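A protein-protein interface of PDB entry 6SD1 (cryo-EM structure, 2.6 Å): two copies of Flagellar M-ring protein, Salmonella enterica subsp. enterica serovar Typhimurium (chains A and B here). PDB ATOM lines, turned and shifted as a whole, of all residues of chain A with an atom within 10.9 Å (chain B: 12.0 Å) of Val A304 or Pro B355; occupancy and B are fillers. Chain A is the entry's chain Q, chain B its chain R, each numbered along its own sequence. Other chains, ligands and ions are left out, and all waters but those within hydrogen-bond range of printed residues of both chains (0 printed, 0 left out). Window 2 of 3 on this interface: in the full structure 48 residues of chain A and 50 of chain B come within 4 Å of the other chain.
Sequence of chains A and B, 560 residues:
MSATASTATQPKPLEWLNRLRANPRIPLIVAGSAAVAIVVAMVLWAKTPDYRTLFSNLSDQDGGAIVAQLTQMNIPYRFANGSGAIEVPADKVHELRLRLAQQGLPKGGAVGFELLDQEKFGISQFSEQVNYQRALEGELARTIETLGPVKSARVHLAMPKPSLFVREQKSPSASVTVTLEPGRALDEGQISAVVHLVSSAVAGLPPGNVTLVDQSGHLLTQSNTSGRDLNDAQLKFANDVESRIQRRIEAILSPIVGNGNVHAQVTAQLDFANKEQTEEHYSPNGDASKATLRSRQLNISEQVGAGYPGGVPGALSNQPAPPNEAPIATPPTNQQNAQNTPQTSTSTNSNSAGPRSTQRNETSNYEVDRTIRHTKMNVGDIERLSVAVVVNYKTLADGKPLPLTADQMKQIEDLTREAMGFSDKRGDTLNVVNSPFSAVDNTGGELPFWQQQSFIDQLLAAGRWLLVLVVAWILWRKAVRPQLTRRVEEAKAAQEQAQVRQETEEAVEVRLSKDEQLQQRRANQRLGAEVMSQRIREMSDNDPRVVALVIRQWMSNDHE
O of Glu A302 is in hydrogen-bond range of N of Thr B358 (2.7 Å).
The backbone carbonyl oxygen of Arg B356 sits close to the backbone carbonyl oxygen of Glu A302 (3.4 Å).
Among the printed residues, 7 pairs touch across the chains.
Among the printed residues, no Asp or Glu carboxylate lies within 4 Å of a Lys or Arg side-chain nitrogen of the other chain.
Among the printed residues, merely in contact across the chains: Ser A301 with Thr B358 (3.5 Å), Glu A302 with Ser B357 (3.3 Å), Gln A303 with Arg B356 (3.98 Å), Val A304 with Pro B355 (3.9 Å) and Val A304 with Arg B356 (3.9 Å).
Of chain A, only Val A304 comes within 4 Å of Pro B355.
Glu A302 touches three residues of chain B.
No residue of chain B comes within 4 Å of Pro A355.
No residue of chain B comes within 4 Å of Arg A356.
No residue of chain B comes within 4 Å of Ser A357.
Ser B357 touches one residue of chain A.
Of the printed residues of chain A, Arg B356 touches Glu A302, Gln A303 and Val A304.
Of the printed residues of chain B, Ser A301 touches Thr B358 (3.5 Å).
Of the printed residues of chain A, Thr B358 touches Ser A301 (3.5 Å) and Glu A302 (2.7 Å).
The nearest residue of chain A that does not touch Pro B355 is Gln A303 (6.3 Å).
The nearest printed residue of chain B that does not touch Ser A301 is Gln B359 (4.4 Å).
The backbone carbonyl oxygen (O) of Ser A301 lies within hydrogen-bond range of the backbone NH (N) of Gln A359, 3.0 Å away.
The side-chain carboxylate (OE2) of Glu A302 is in salt-bridge range of the guanidinium group (NH2) of Arg A356.
The backbone carbonyl oxygen (O) of Ser A357 is in hydrogen-bond range of the backbone NH (N) of Gln A303 (2.8 Å).
The guanidinium group of Arg B356 is in salt-bridge range of the side-chain carboxylate of Glu B302 (3.5 Å).
The backbone NH of Gln B303 sits at hydrogen-bond distance from the backbone carbonyl oxygen of Ser B357 (2.8 Å).
Ser A301 touches Thr B358, but with the chains exchanged Thr A358 does not touch Ser B301 (12.8 Å).
Glu A302 touches Thr B358, but with the chains exchanged Thr A358 does not touch Glu B302 (13.8 Å).
Val A304 touches Pro B355, but with the chains exchanged Pro A355 does not touch Val B304 (12.8 Å).
Val A304 touches Arg B356, but with the chains exchanged Arg A356 does not touch Val B304 (13.8 Å).
Positions printed for both chains: 301, 302, 303, 304, 355, 356, 357, 358 and 359.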
ATOM      1  N   SER A 301      13.621  16.549  -1.608  1.00  0.00           N
ATOM      2  CA  SER A 301      13.944  17.526  -0.582  1.00  0.00           C
ATOM      3  C   SER A 301      13.881  18.925  -1.178  1.00  0.00           C
ATOM      4  O   SER A 301      14.015  19.106  -2.391  1.00  0.00           O
ATOM      5  CB  SER A 301      15.330  17.265   0.011  1.00  0.00           C
ATOM      6  OG  SER A 301      15.648  18.222   1.004  1.00  0.00           O
ATOM      7  N   GLU A 302      13.668  19.917  -0.316  1.00  0.00           N
ATOM      8  CA  GLU A 302      13.509  21.292  -0.784  1.00  0.00           C
ATOM      9  C   GLU A 302      13.648  22.233   0.403  1.00  0.00           C
ATOM     10  O   GLU A 302      12.919  22.097   1.389  1.00  0.00           O
ATOM     11  CB  GLU A 302      12.162  21.472  -1.470  1.00  0.00           C
ATOM     12  CG  GLU A 302      11.820  22.908  -1.782  1.00  0.00           C
ATOM     13  CD  GLU A 302      10.727  23.026  -2.819  1.00  0.00           C
ATOM     14  OE1 GLU A 302      10.343  21.987  -3.396  1.00  0.00           O
ATOM     15  OE2 GLU A 302      10.250  24.155  -3.056  1.00  0.00           O
ATOM     16  N   GLN A 303      14.573  23.184   0.305  1.00  0.00           N
ATOM     17  CA  GLN A 303      14.756  24.220   1.311  1.00  0.00           C
ATOM     18  C   GLN A 303      14.596  25.583   0.656  1.00  0.00           C
ATOM     19  O   GLN A 303      14.912  25.748  -0.526  1.00  0.00           O
ATOM     20  CB  GLN A 303      16.127  24.109   1.976  1.00  0.00           C
ATOM     21  CG  GLN A 303      16.507  22.698   2.373  1.00  0.00           C
ATOM     22  CD  GLN A 303      17.813  22.645   3.134  1.00  0.00           C
ATOM     23  OE1 GLN A 303      18.115  23.531   3.933  1.00  0.00           O
ATOM     24  NE2 GLN A 303      18.599  21.606   2.886  1.00  0.00           N
ATOM     25  N   VAL A 304      14.099  26.548   1.420  1.00  0.00           N
ATOM     26  CA  VAL A 304      13.917  27.904   0.920  1.00  0.00           C
ATOM     27  C   VAL A 304      14.446  28.901   1.942  1.00  0.00           C
ATOM     28  O   VAL A 304      15.228  28.544   2.822  1.00  0.00           O
ATOM     29  CB  VAL A 304      12.444  28.188   0.591  1.00  0.00           C
ATOM     30  CG1 VAL A 304      12.226  29.677   0.388  1.00  0.00           C
ATOM     31  CG2 VAL A 304      12.017  27.415  -0.645  1.00  0.00           C
ATOM     32  N   PRO A 355      18.131  31.387  -2.333  1.00  0.00           N
ATOM     33  CA  PRO A 355      18.611  30.275  -1.507  1.00  0.00           C
ATOM     34  C   PRO A 355      17.633  29.102  -1.506  1.00  0.00           C
ATOM     35  O   PRO A 355      17.012  28.814  -0.485  1.00  0.00           O
ATOM     36  CB  PRO A 355      18.726  30.898  -0.117  1.00  0.00           C
ATOM     37  CG  PRO A 355      17.696  31.973  -0.109  1.00  0.00           C
ATOM     38  CD  PRO A 355      17.572  32.483  -1.520  1.00  0.00           C
ATOM     39  N   ARG A 356      17.510  28.433  -2.647  1.00  0.00           N
ATOM     40  CA  ARG A 356      16.533  27.367  -2.849  1.00  0.00           C
ATOM     41  C   ARG A 356      17.287  26.074  -3.149  1.00  0.00           C
ATOM     42  O   ARG A 356      17.540  25.737  -4.305  1.00  0.00           O
ATOM     43  CB  ARG A 356      15.568  27.733  -3.972  1.00  0.00           C
ATOM     44  CG  ARG A 356      14.421  26.761  -4.150  1.00  0.00           C
ATOM     45  CD  ARG A 356      13.482  27.224  -5.248  1.00  0.00           C
ATOM     46  NE  ARG A 356      12.220  26.492  -5.226  1.00  0.00           N
ATOM     47  CZ  ARG A 356      11.277  26.601  -6.155  1.00  0.00           C
ATOM     48  NH1 ARG A 356      11.451  27.412  -7.188  1.00  0.00           N
ATOM     49  NH2 ARG A 356      10.158  25.896  -6.053  1.00  0.00           N
ATOM     50  N   SER A 357      17.640  25.348  -2.090  1.00  0.00           N
ATOM     51  CA  SER A 357      18.362  24.081  -2.202  1.00  0.00           C
ATOM     52  C   SER A 357      17.349  22.973  -2.463  1.00  0.00           C
ATOM     53  O   SER A 357      16.600  22.564  -1.577  1.00  0.00           O
ATOM     54  CB  SER A 357      19.175  23.817  -0.942  1.00  0.00           C
ATOM     55  OG  SER A 357      19.845  22.572  -1.014  1.00  0.00           O
ATOM     56  N   THR A 358      17.332  22.476  -3.695  1.00  0.00           N
ATOM     57  CA  THR A 358      16.361  21.477  -4.109  1.00  0.00           C
ATOM     58  C   THR A 358      17.054  20.173  -4.500  1.00  0.00           C
ATOM     59  O   THR A 358      18.046  20.155  -5.229  1.00  0.00           O
ATOM     60  CB  THR A 358      15.518  22.009  -5.268  1.00  0.00           C
ATOM     61  OG1 THR A 358      14.690  23.081  -4.803  1.00  0.00           O
ATOM     62  CG2 THR A 358      14.635  20.914  -5.844  1.00  0.00           C
ATOM     63  N   GLN A 359      16.513  19.067  -3.996  1.00  0.00           N
ATOM     64  CA  GLN A 359      17.034  17.739  -4.289  1.00  0.00           C
ATOM     65  C   GLN A 359      15.893  16.881  -4.813  1.00  0.00           C
ATOM     66  O   GLN A 359      14.730  17.138  -4.501  1.00  0.00           O
ATOM     67  CB  GLN A 359      17.655  17.103  -3.039  1.00  0.00           C
ATOM     68  CG  GLN A 359      18.513  15.886  -3.316  1.00  0.00           C
ATOM     69  CD  GLN A 359      19.595  15.692  -2.276  1.00  0.00           C
ATOM     70  OE1 GLN A 359      19.384  15.939  -1.089  1.00  0.00           O
ATOM     71  NE2 GLN A 359      20.767  15.248  -2.718  1.00  0.00           N
ATOM     72  N   SER B 301       8.099  15.219   5.768  1.00  0.00           N
ATOM     73  CA  SER B 301       8.556  16.190   6.748  1.00  0.00           C
ATOM     74  C   SER B 301       8.313  17.596   6.217  1.00  0.00           C
ATOM     75  O   SER B 301       8.203  17.809   5.008  1.00  0.00           O
ATOM     76  CB  SER B 301      10.040  15.994   7.068  1.00  0.00           C
ATOM     77  OG  SER B 301      10.487  16.947   8.014  1.00  0.00           O
ATOM     78  N   GLU B 302       8.224  18.558   7.134  1.00  0.00           N
ATOM     79  CA  GLU B 302       7.911  19.932   6.747  1.00  0.00           C
ATOM     80  C   GLU B 302       8.206  20.853   7.923  1.00  0.00           C
ATOM     81  O   GLU B 302       7.598  20.709   8.986  1.00  0.00           O
ATOM     82  CB  GLU B 302       6.456  20.049   6.314  1.00  0.00           C
ATOM     83  CG  GLU B 302       5.997  21.469   6.089  1.00  0.00           C
ATOM     84  CD  GLU B 302       4.774  21.545   5.205  1.00  0.00           C
ATOM     85  OE1 GLU B 302       4.358  20.492   4.677  1.00  0.00           O
ATOM     86  OE2 GLU B 302       4.227  22.654   5.038  1.00  0.00           O
ATOM     87  N   GLN B 303       9.124  21.792   7.727  1.00  0.00           N
ATOM     88  CA  GLN B 303       9.428  22.821   8.710  1.00  0.00           C
ATOM     89  C   GLN B 303       9.090  24.182   8.124  1.00  0.00           C
ATOM     90  O   GLN B 303       9.299  24.417   6.931  1.00  0.00           O
ATOM     91  CB  GLN B 303      10.898  22.774   9.126  1.00  0.00           C
ATOM     92  CG  GLN B 303      11.411  21.380   9.419  1.00  0.00           C
ATOM     93  CD  GLN B 303      12.854  21.380   9.872  1.00  0.00           C
ATOM     94  OE1 GLN B 303      13.294  22.286  10.578  1.00  0.00           O
ATOM     95  NE2 GLN B 303      13.602  20.363   9.462  1.00  0.00           N
ATOM     96  N   VAL B 304       8.562  25.070   8.960  1.00  0.00           N
ATOM     97  CA  VAL B 304       8.210  26.414   8.526  1.00  0.00           C
ATOM     98  C   VAL B 304       8.769  27.432   9.508  1.00  0.00           C
ATOM     99  O   VAL B 304       9.786  27.186  10.157  1.00  0.00           O
ATOM    100  CB  VAL B 304       6.690  26.574   8.378  1.00  0.00           C
ATOM    101  CG1 VAL B 304       6.330  28.036   8.198  1.00  0.00           C
ATOM    102  CG2 VAL B 304       6.181  25.753   7.206  1.00  0.00           C
ATOM    103  N   PRO B 355      11.790  30.270   4.695  1.00  0.00           N
ATOM    104  CA  PRO B 355      12.401  29.154   5.423  1.00  0.00           C
ATOM    105  C   PRO B 355      11.451  27.966   5.551  1.00  0.00           C
ATOM    106  O   PRO B 355      10.894  27.730   6.621  1.00  0.00           O
ATOM    107  CB  PRO B 355      12.711  29.762   6.791  1.00  0.00           C
ATOM    108  CG  PRO B 355      11.686  30.824   6.965  1.00  0.00           C
ATOM    109  CD  PRO B 355      11.349  31.349   5.595  1.00  0.00           C
ATOM    110  N   ARG B 356      11.277  27.225   4.461  1.00  0.00           N
ATOM    111  CA  ARG B 356      10.309  26.135   4.386  1.00  0.00           C
ATOM    112  C   ARG B 356      11.035  24.875   3.918  1.00  0.00           C
ATOM    113  O   ARG B 356      11.051  24.554   2.730  1.00  0.00           O
ATOM    114  CB  ARG B 356       9.163  26.506   3.452  1.00  0.00           C
ATOM    115  CG  ARG B 356       7.988  25.552   3.499  1.00  0.00           C
ATOM    116  CD  ARG B 356       6.877  26.016   2.574  1.00  0.00           C
ATOM    117  NE  ARG B 356       5.663  25.222   2.744  1.00  0.00           N
ATOM    118  CZ  ARG B 356       4.592  25.320   1.965  1.00  0.00           C
ATOM    119  NH1 ARG B 356       4.580  26.180   0.955  1.00  0.00           N
ATOM    120  NH2 ARG B 356       3.532  24.558   2.193  1.00  0.00           N
ATOM    121  N   SER B 357      11.632  24.158   4.869  1.00  0.00           N
ATOM    122  CA  SER B 357      12.352  22.917   4.586  1.00  0.00           C
ATOM    123  C   SER B 357      11.332  21.794   4.460  1.00  0.00           C
ATOM    124  O   SER B 357      10.719  21.366   5.437  1.00  0.00           O
ATOM    125  CB  SER B 357      13.375  22.626   5.676  1.00  0.00           C
ATOM    126  OG  SER B 357      14.363  23.639   5.728  1.00  0.00           O
ATOM    127  N   THR B 358      11.152  21.303   3.239  1.00  0.00           N
ATOM    128  CA  THR B 358      10.156  20.283   2.961  1.00  0.00           C
ATOM    129  C   THR B 358      10.813  19.021   2.406  1.00  0.00           C
ATOM    130  O   THR B 358      11.620  19.061   1.478  1.00  0.00           O
ATOM    131  CB  THR B 358       9.108  20.818   1.985  1.00  0.00           C
ATOM    132  OG1 THR B 358       8.318  21.820   2.636  1.00  0.00           O
ATOM    133  CG2 THR B 358       8.199  19.701   1.509  1.00  0.00           C
ATOM    134  N   GLN B 359      10.454  17.884   2.998  1.00  0.00           N
ATOM    135  CA  GLN B 359      10.962  16.590   2.568  1.00  0.00           C
ATOM    136  C   GLN B 359       9.780  15.700   2.215  1.00  0.00           C
ATOM    137  O   GLN B 359       8.681  15.892   2.738  1.00  0.00           O
ATOM    138  CB  GLN B 359      11.814  15.939   3.664  1.00  0.00           C
ATOM    139  CG  GLN B 359      12.738  14.845   3.170  1.00  0.00           C
ATOM    140  CD  GLN B 359      13.983  14.706   4.024  1.00  0.00           C
ATOM    141  OE1 GLN B 359      13.941  14.901   5.238  1.00  0.00           O
ATOM    142  NE2 GLN B 359      15.099  14.364   3.391  1.00  0.00           N
